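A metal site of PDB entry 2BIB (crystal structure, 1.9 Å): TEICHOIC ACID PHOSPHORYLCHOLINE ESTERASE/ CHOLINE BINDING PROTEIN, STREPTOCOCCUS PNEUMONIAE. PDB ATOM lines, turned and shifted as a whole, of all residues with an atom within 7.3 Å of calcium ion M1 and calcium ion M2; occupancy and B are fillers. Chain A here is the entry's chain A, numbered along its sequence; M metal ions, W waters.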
ATOM      1  N   THR A  34      31.681  17.426  24.191  1.00  0.00           N
ATOM      2  CA  THR A  34      30.318  17.395  24.776  1.00  0.00           C
ATOM      3  C   THR A  34      29.278  16.663  23.913  1.00  0.00           C
ATOM      4  O   THR A  34      28.099  16.650  24.268  1.00  0.00           O
ATOM      5  CB  THR A  34      29.840  18.832  25.043  1.00  0.00           C
ATOM      6  OG1 THR A  34      29.591  19.511  23.795  1.00  0.00           O
ATOM      7  CG2 THR A  34      30.877  19.571  25.842  1.00  0.00           C
ATOM      8  N   GLY A  35      29.719  16.067  22.815  1.00  0.00           N
ATOM      9  CA  GLY A  35      28.842  15.318  21.942  1.00  0.00           C
ATOM     10  C   GLY A  35      27.931  16.124  21.043  1.00  0.00           C
ATOM     11  O   GLY A  35      27.809  17.344  21.181  1.00  0.00           O
ATOM     12  N   GLU A  36      27.277  15.443  20.108  1.00  0.00           N
ATOM     13  CA  GLU A  36      26.299  16.056  19.215  1.00  0.00           C
ATOM     14  C   GLU A  36      25.060  16.521  19.964  1.00  0.00           C
ATOM     15  O   GLU A  36      24.578  15.833  20.886  1.00  0.00           O
ATOM     16  CB  GLU A  36      25.881  15.051  18.106  1.00  0.00           C
ATOM     17  CG  GLU A  36      24.991  15.642  17.013  1.00  0.00           C
ATOM     18  CD  GLU A  36      25.710  16.738  16.226  1.00  0.00           C
ATOM     19  OE1 GLU A  36      26.662  16.396  15.494  1.00  0.00           O
ATOM     20  OE2 GLU A  36      25.317  17.940  16.355  1.00  0.00           O
ATOM     21  N   ASP A  37      24.559  17.700  19.586  1.00  0.00           N
ATOM     22  CA  ASP A  37      23.334  18.277  20.148  1.00  0.00           C
ATOM     23  C   ASP A  37      22.195  18.270  19.144  1.00  0.00           C
ATOM     24  O   ASP A  37      22.439  18.289  17.922  1.00  0.00           O
ATOM     25  CB  ASP A  37      23.536  19.714  20.643  1.00  0.00           C
ATOM     26  CG  ASP A  37      23.805  20.714  19.505  1.00  0.00           C
ATOM     27  OD1 ASP A  37      24.322  20.327  18.429  1.00  0.00           O
ATOM     28  OD2 ASP A  37      23.552  21.932  19.617  1.00  0.00           O
ATOM     29  N   TYR A  38      20.966  18.283  19.655  1.00  0.00           N
ATOM     30  CA  TYR A  38      19.778  18.466  18.824  1.00  0.00           C
ATOM     31  C   TYR A  38      19.857  19.660  17.884  1.00  0.00           C
ATOM     32  O   TYR A  38      19.563  19.544  16.689  1.00  0.00           O
ATOM     33  CB  TYR A  38      18.557  18.644  19.728  1.00  0.00           C
ATOM     34  CG  TYR A  38      18.119  17.365  20.358  1.00  0.00           C
ATOM     35  CD1 TYR A  38      18.315  17.145  21.718  1.00  0.00           C
ATOM     36  CD2 TYR A  38      17.496  16.371  19.607  1.00  0.00           C
ATOM     37  CE1 TYR A  38      17.906  15.954  22.318  1.00  0.00           C
ATOM     38  CE2 TYR A  38      17.086  15.179  20.193  1.00  0.00           C
ATOM     39  CZ  TYR A  38      17.289  14.989  21.552  1.00  0.00           C
ATOM     40  OH  TYR A  38      16.887  13.820  22.144  1.00  0.00           O
ATOM     41  N   ASP A  39      20.256  20.802  18.431  1.00  0.00           N
ATOM     42  CA  ASP A  39      20.271  22.064  17.703  1.00  0.00           C
ATOM     43  C   ASP A  39      21.116  22.019  16.436  1.00  0.00           C
ATOM     44  O   ASP A  39      22.090  21.265  16.349  1.00  0.00           O
ATOM     45  CB  ASP A  39      20.739  23.207  18.616  1.00  0.00           C
ATOM     46  CG  ASP A  39      20.295  24.561  18.121  1.00  0.00           C
ATOM     47  OD1 ASP A  39      20.888  25.581  18.554  1.00  0.00           O
ATOM     48  OD2 ASP A  39      19.363  24.711  17.307  1.00  0.00           O
ATOM     49  N   PHE A  40      20.734  22.852  15.476  1.00  0.00           N
ATOM     50  CA  PHE A  40      21.490  23.045  14.227  1.00  0.00           C
ATOM     51  C   PHE A  40      20.980  24.332  13.578  1.00  0.00           C
ATOM     52  O   PHE A  40      19.851  24.730  13.874  1.00  0.00           O
ATOM     53  CB  PHE A  40      21.249  21.858  13.282  1.00  0.00           C
ATOM     54  CG  PHE A  40      19.788  21.627  12.953  1.00  0.00           C
ATOM     55  CD1 PHE A  40      19.198  22.239  11.840  1.00  0.00           C
ATOM     56  CD2 PHE A  40      19.019  20.788  13.743  1.00  0.00           C
ATOM     57  CE1 PHE A  40      17.856  22.030  11.531  1.00  0.00           C
ATOM     58  CE2 PHE A  40      17.670  20.557  13.441  1.00  0.00           C
ATOM     59  CZ  PHE A  40      17.089  21.178  12.335  1.00  0.00           C
ATOM     60  N   PRO A  41      21.759  24.992  12.714  1.00  0.00           N
ATOM     61  CA  PRO A  41      21.252  26.156  11.991  1.00  0.00           C
ATOM     62  C   PRO A  41      20.418  25.755  10.777  1.00  0.00           C
ATOM     63  O   PRO A  41      20.804  24.839  10.062  1.00  0.00           O
ATOM     64  CB  PRO A  41      22.535  26.893  11.561  1.00  0.00           C
ATOM     65  CG  PRO A  41      23.608  25.830  11.515  1.00  0.00           C
ATOM     66  CD  PRO A  41      23.160  24.676  12.391  1.00  0.00           C
ATOM     67  N   ILE A  54      25.225  18.883   7.415  1.00  0.00           N
ATOM     68  CA  ILE A  54      24.950  19.320   8.797  1.00  0.00           C
ATOM     69  C   ILE A  54      24.075  18.253   9.481  1.00  0.00           C
ATOM     70  O   ILE A  54      23.043  17.847   8.915  1.00  0.00           O
ATOM     71  CB  ILE A  54      24.243  20.696   8.844  1.00  0.00           C
ATOM     72  CG1 ILE A  54      25.197  21.835   8.426  1.00  0.00           C
ATOM     73  CG2 ILE A  54      23.637  20.965  10.236  1.00  0.00           C
ATOM     74  CD1 ILE A  54      24.488  23.178   8.232  1.00  0.00           C
ATOM     75  N   GLU A  55      24.475  17.812  10.672  1.00  0.00           N
ATOM     76  CA  GLU A  55      23.730  16.769  11.431  1.00  0.00           C
ATOM     77  C   GLU A  55      22.299  17.183  11.852  1.00  0.00           C
ATOM     78  O   GLU A  55      22.117  18.235  12.475  1.00  0.00           O
ATOM     79  CB  GLU A  55      24.523  16.340  12.677  1.00  0.00           C
ATOM     80  CG  GLU A  55      23.946  15.139  13.415  1.00  0.00           C
ATOM     81  CD  GLU A  55      23.954  13.904  12.544  1.00  0.00           C
ATOM     82  OE1 GLU A  55      25.031  13.290  12.396  1.00  0.00           O
ATOM     83  OE2 GLU A  55      22.912  13.583  11.976  1.00  0.00           O
ATOM     84  N   THR A  56      21.302  16.359  11.521  1.00  0.00           N
ATOM     85  CA  THR A  56      19.923  16.532  12.038  1.00  0.00           C
ATOM     86  C   THR A  56      19.263  15.223  12.518  1.00  0.00           C
ATOM     87  O   THR A  56      18.063  15.215  12.866  1.00  0.00           O
ATOM     88  CB  THR A  56      18.978  17.167  10.981  1.00  0.00           C
ATOM     89  OG1 THR A  56      18.858  16.283   9.864  1.00  0.00           O
ATOM     90  CG2 THR A  56      19.545  18.477  10.389  1.00  0.00           C
ATOM     91  N   VAL A  61      22.432  12.201  18.050  1.00  0.00           N
ATOM     92  CA  VAL A  61      22.387  13.200  19.147  1.00  0.00           C
ATOM     93  C   VAL A  61      22.780  12.598  20.504  1.00  0.00           C
ATOM     94  O   VAL A  61      22.195  11.589  20.954  1.00  0.00           O
ATOM     95  CB  VAL A  61      20.990  13.868  19.250  1.00  0.00           C
ATOM     96  CG1 VAL A  61      20.900  14.836  20.447  1.00  0.00           C
ATOM     97  CG2 VAL A  61      20.654  14.594  17.974  1.00  0.00           C
ATOM     98  N   THR A  63      22.798  14.488  23.383  1.00  0.00           N
ATOM     99  CA  THR A  63      22.272  15.365  24.442  1.00  0.00           C
ATOM    100  C   THR A  63      21.624  14.591  25.610  1.00  0.00           C
ATOM    101  O   THR A  63      21.985  14.814  26.758  1.00  0.00           O
ATOM    102  CB  THR A  63      21.264  16.365  23.851  1.00  0.00           C
ATOM    103  OG1 THR A  63      21.908  17.206  22.873  1.00  0.00           O
ATOM    104  CG2 THR A  63      20.769  17.332  24.936  1.00  0.00           C
ATOM    105  N   SER A  88      30.226  19.729  15.176  1.00  0.00           N
ATOM    106  CA  SER A  88      29.017  19.622  15.972  1.00  0.00           C
ATOM    107  C   SER A  88      29.021  18.401  16.905  1.00  0.00           C
ATOM    108  O   SER A  88      28.436  18.438  17.976  1.00  0.00           O
ATOM    109  CB  SER A  88      27.794  19.578  15.055  1.00  0.00           C
ATOM    110  OG  SER A  88      27.771  18.371  14.311  1.00  0.00           O
ATOM    111  N   ASP A  89      29.676  17.318  16.492  1.00  0.00           N
ATOM    112  CA  ASP A  89      29.670  16.071  17.262  1.00  0.00           C
ATOM    113  C   ASP A  89      30.659  16.092  18.439  1.00  0.00           C
ATOM    114  O   ASP A  89      30.794  15.097  19.166  1.00  0.00           O
ATOM    115  CB  ASP A  89      29.899  14.835  16.373  1.00  0.00           C
ATOM    116  CG  ASP A  89      31.229  14.865  15.640  1.00  0.00           C
ATOM    117  OD1 ASP A  89      31.478  15.864  14.934  1.00  0.00           O
ATOM    118  OD2 ASP A  89      32.095  13.952  15.707  1.00  0.00           O
ATOM    119  N   ILE A  91      31.533  19.829  19.853  1.00  0.00           N
ATOM    120  CA  ILE A  91      31.163  21.108  20.483  1.00  0.00           C
ATOM    121  C   ILE A  91      29.661  21.247  20.763  1.00  0.00           C
ATOM    122  O   ILE A  91      29.218  22.204  21.401  1.00  0.00           O
ATOM    123  CB  ILE A  91      31.638  22.272  19.543  1.00  0.00           C
ATOM    124  CG1 ILE A  91      31.954  23.564  20.329  1.00  0.00           C
ATOM    125  CG2 ILE A  91      30.630  22.491  18.375  1.00  0.00           C
ATOM    126  CD1 ILE A  91      32.776  24.636  19.490  1.00  0.00           C
ATOM    127  N   GLY A  92      28.869  20.288  20.289  1.00  0.00           N
ATOM    128  CA  GLY A  92      27.428  20.449  20.221  1.00  0.00           C
ATOM    129  C   GLY A  92      26.710  20.873  21.484  1.00  0.00           C
ATOM    130  O   GLY A  92      25.901  21.815  21.450  1.00  0.00           O
ATOM    131  N   ASN A  93      26.976  20.193  22.591  1.00  0.00           N
ATOM    132  CA  ASN A  93      26.269  20.511  23.835  1.00  0.00           C
ATOM    133  C   ASN A  93      26.913  21.532  24.777  1.00  0.00           C
ATOM    134  O   ASN A  93      26.457  21.678  25.907  1.00  0.00           O
ATOM    135  CB  ASN A  93      25.933  19.246  24.591  1.00  0.00           C
ATOM    136  CG  ASN A  93      24.950  18.401  23.850  1.00  0.00           C
ATOM    137  OD1 ASN A  93      23.794  18.773  23.694  1.00  0.00           O
ATOM    138  ND2 ASN A  93      25.408  17.257  23.350  1.00  0.00           N
ATOM    139  N   VAL A  94      27.938  22.237  24.324  1.00  0.00           N
ATOM    140  CA  VAL A  94      28.640  23.179  25.210  1.00  0.00           C
ATOM    141  C   VAL A  94      27.714  24.275  25.712  1.00  0.00           C
ATOM    142  O   VAL A  94      27.659  24.535  26.910  1.00  0.00           O
ATOM    143  CB  VAL A  94      29.867  23.840  24.564  1.00  0.00           C
ATOM    144  CG1 VAL A  94      30.540  24.796  25.563  1.00  0.00           C
ATOM    145  CG2 VAL A  94      30.879  22.784  24.101  1.00  0.00           C
ATOM    146  N   ASP A  95      26.992  24.926  24.792  1.00  0.00           N
ATOM    147  CA  ASP A  95      26.126  26.020  25.215  1.00  0.00           C
ATOM    148  C   ASP A  95      25.016  25.528  26.146  1.00  0.00           C
ATOM    149  O   ASP A  95      24.730  26.162  27.163  1.00  0.00           O
ATOM    150  CB  ASP A  95      25.581  26.821  24.026  1.00  0.00           C
ATOM    151  CG  ASP A  95      24.825  25.970  23.027  1.00  0.00           C
ATOM    152  OD1 ASP A  95      25.437  25.042  22.449  1.00  0.00           O
ATOM    153  OD2 ASP A  95      23.633  26.199  22.740  1.00  0.00           O
ATOM    154  N   GLU A  96      24.410  24.381  25.815  1.00  0.00           N
ATOM    155  CA  GLU A  96      23.381  23.791  26.696  1.00  0.00           C
ATOM    156  C   GLU A  96      23.961  23.489  28.092  1.00  0.00           C
ATOM    157  O   GLU A  96      23.302  23.708  29.111  1.00  0.00           O
ATOM    158  CB  GLU A  96      22.815  22.514  26.070  1.00  0.00           C
ATOM    159  CG  GLU A  96      21.957  22.728  24.822  1.00  0.00           C
ATOM    160  CD  GLU A  96      22.774  22.821  23.524  1.00  0.00           C
ATOM    161  OE1 GLU A  96      24.035  22.724  23.566  1.00  0.00           O
ATOM    162  OE2 GLU A  96      22.154  23.011  22.456  1.00  0.00           O
ATOM    163  N   LEU A  97      25.198  23.004  28.143  1.00  0.00           N
ATOM    164  CA  LEU A  97      25.861  22.746  29.431  1.00  0.00           C
ATOM    165  C   LEU A  97      26.128  24.026  30.211  1.00  0.00           C
ATOM    166  O   LEU A  97      25.876  24.077  31.432  1.00  0.00           O
ATOM    167  CB  LEU A  97      27.151  21.949  29.234  1.00  0.00           C
ATOM    168  CG  LEU A  97      26.908  20.460  28.917  1.00  0.00           C
ATOM    169  CD1 LEU A  97      28.110  19.877  28.172  1.00  0.00           C
ATOM    170  CD2 LEU A  97      26.587  19.664  30.186  1.00  0.00           C
ATOM    171  N   ASP A 124      28.162  23.362  10.048  1.00  0.00           N
ATOM    172  CA  ASP A 124      27.759  24.310  11.089  1.00  0.00           C
ATOM    173  C   ASP A 124      28.846  24.511  12.160  1.00  0.00           C
ATOM    174  O   ASP A 124      28.539  24.676  13.344  1.00  0.00           O
ATOM    175  CB  ASP A 124      26.469  23.849  11.767  1.00  0.00           C
ATOM    176  CG  ASP A 124      26.568  22.448  12.362  1.00  0.00           C
ATOM    177  OD1 ASP A 124      27.509  21.678  12.043  1.00  0.00           O
ATOM    178  OD2 ASP A 124      25.736  22.059  13.200  1.00  0.00           O
ATOM    179  N   TYR A 127      28.539  28.115  13.649  1.00  0.00           N
ATOM    180  CA  TYR A 127      27.365  28.149  14.520  1.00  0.00           C
ATOM    181  C   TYR A 127      27.694  27.582  15.905  1.00  0.00           C
ATOM    182  O   TYR A 127      27.351  28.196  16.938  1.00  0.00           O
ATOM    183  CB  TYR A 127      26.189  27.418  13.872  1.00  0.00           C
ATOM    184  CG  TYR A 127      24.920  27.475  14.694  1.00  0.00           C
ATOM    185  CD1 TYR A 127      24.100  28.609  14.691  1.00  0.00           C
ATOM    186  CD2 TYR A 127      24.523  26.382  15.468  1.00  0.00           C
ATOM    187  CE1 TYR A 127      22.921  28.669  15.462  1.00  0.00           C
ATOM    188  CE2 TYR A 127      23.346  26.420  16.218  1.00  0.00           C
ATOM    189  CZ  TYR A 127      22.545  27.563  16.208  1.00  0.00           C
ATOM    190  OH  TYR A 127      21.390  27.590  16.972  1.00  0.00           O
ATOM    191  N   GLY A 128      28.402  26.464  15.938  1.00  0.00           N
ATOM    192  CA  GLY A 128      28.719  25.807  17.185  1.00  0.00           C
ATOM    193  C   GLY A 128      29.729  26.599  17.997  1.00  0.00           C
ATOM    194  O   GLY A 128      29.611  26.716  19.220  1.00  0.00           O
ATOM    195  N   LYS A 131      28.158  29.817  19.469  1.00  0.00           N
ATOM    196  CA  LYS A 131      27.324  29.412  20.583  1.00  0.00           C
ATOM    197  C   LYS A 131      28.136  29.335  21.857  1.00  0.00           C
ATOM    198  O   LYS A 131      27.647  29.739  22.918  1.00  0.00           O
ATOM    199  CB  LYS A 131      26.685  28.047  20.286  1.00  0.00           C
ATOM    200  CG  LYS A 131      25.327  28.077  19.596  1.00  0.00           C
ATOM    201  CD  LYS A 131      24.240  28.804  20.407  1.00  0.00           C
ATOM    202  CE  LYS A 131      23.055  29.207  19.522  1.00  0.00           C
ATOM    203  NZ  LYS A 131      21.818  29.502  20.317  1.00  0.00           N
ATOM    204  N   VAL A 335      14.263  15.731  15.148  1.00  0.00           N
ATOM    205  CA  VAL A 335      14.460  17.144  14.801  1.00  0.00           C
ATOM    206  C   VAL A 335      14.762  17.215  13.316  1.00  0.00           C
ATOM    207  O   VAL A 335      15.220  16.225  12.713  1.00  0.00           O
ATOM    208  CB  VAL A 335      15.580  17.872  15.662  1.00  0.00           C
ATOM    209  CG1 VAL A 335      15.176  17.982  17.153  1.00  0.00           C
ATOM    210  CG2 VAL A 335      16.953  17.228  15.502  1.00  0.00           C
HETATM  211 CA    CA M   1      24.301  23.450  21.211  1.00  0.00          CA
HETATM  212 CA    CA M   2      23.660  19.563  16.223  1.00  0.00          CA
HETATM  213  O   HOH W   1      21.796  18.379  15.223  1.00  0.00           O
HETATM  214  O   HOH W   2      24.068  19.864  13.888  1.00  0.00           O
HETATM  215  O   HOH W   3      22.937  25.184  20.300  1.00  0.00           O
HETATM  216  O   HOH W   4      25.092  21.499  15.792  1.00  0.00           O
HETATM  217  O   HOH W   5      25.952  23.904  19.437  1.00  0.00           O
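Within 4 Å of calcium ion M1: Asp 37, Gly 92, Asp 95 and Glu 96.
O of Gly 35 lies within hydrogen-bond range of N of Gly 92, 3.3 Å away.
OD1 of Asp 39 is in hydrogen-bond range of OH of Tyr 127 (2.6 Å).
The side-chain hydroxyl of Ser 88 lies within hydrogen-bond range of the side-chain carboxylate of Glu 36 (2.6 Å).
The backbone carbonyl oxygen (O) of Glu 36 is in hydrogen-bond range of the side-chain amide nitrogen (ND2) of Asn 93 (3.0 Å).
The side-chain carboxylate (OE1) of Glu 36 sits at hydrogen-bond distance from the backbone NH (N) of Asp 89 (3.3 Å).
O of Glu 36 is in hydrogen-bond range of N of Thr 63, 3.3 Å away.
Calcium ion M2 is bound by the backbone carbonyl oxygen (O) of Asp 39 (2.3 Å), the side-chain carboxylate (OE2) of Glu 36 (2.3 Å), water W2 (2.4 Å), water W1 (2.4 Å), the side-chain carboxylate (OD1) of Asp 37 (2.4 Å), water W4 (2.4 Å) and the backbone carbonyl oxygen (O) of Asp 37 (2.4 Å).
Water W3 bridges OD1 of Asp 39 and OD2 of Asp 95.
Water W1 lies within hydrogen-bond range of O of Glu 55 (2.8 Å) and O of Tyr 38 (2.9 Å).
Water W2 lies within hydrogen-bond range of OD2 of Asp 124 (2.8 Å) and O of Glu 55 (2.9 Å).
Calcium ion M1 is bound by the backbone carbonyl oxygen (O) of Gly 92 (2.3 Å), the side-chain carboxylate (OD1) of Asp 95 (2.3 Å), the side-chain carboxylate (OD2) of Asp 37 (2.3 Å), water W3 (2.4 Å), water W5 (2.5 Å), the side-chain carboxylate (OE1) of Glu 96 (2.5 Å) and the side-chain carboxylate (OE2) of Glu 96 (2.5 Å).
The nearest printed residue that does not touch calcium ion M2 is Tyr 38 (4.1 Å).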
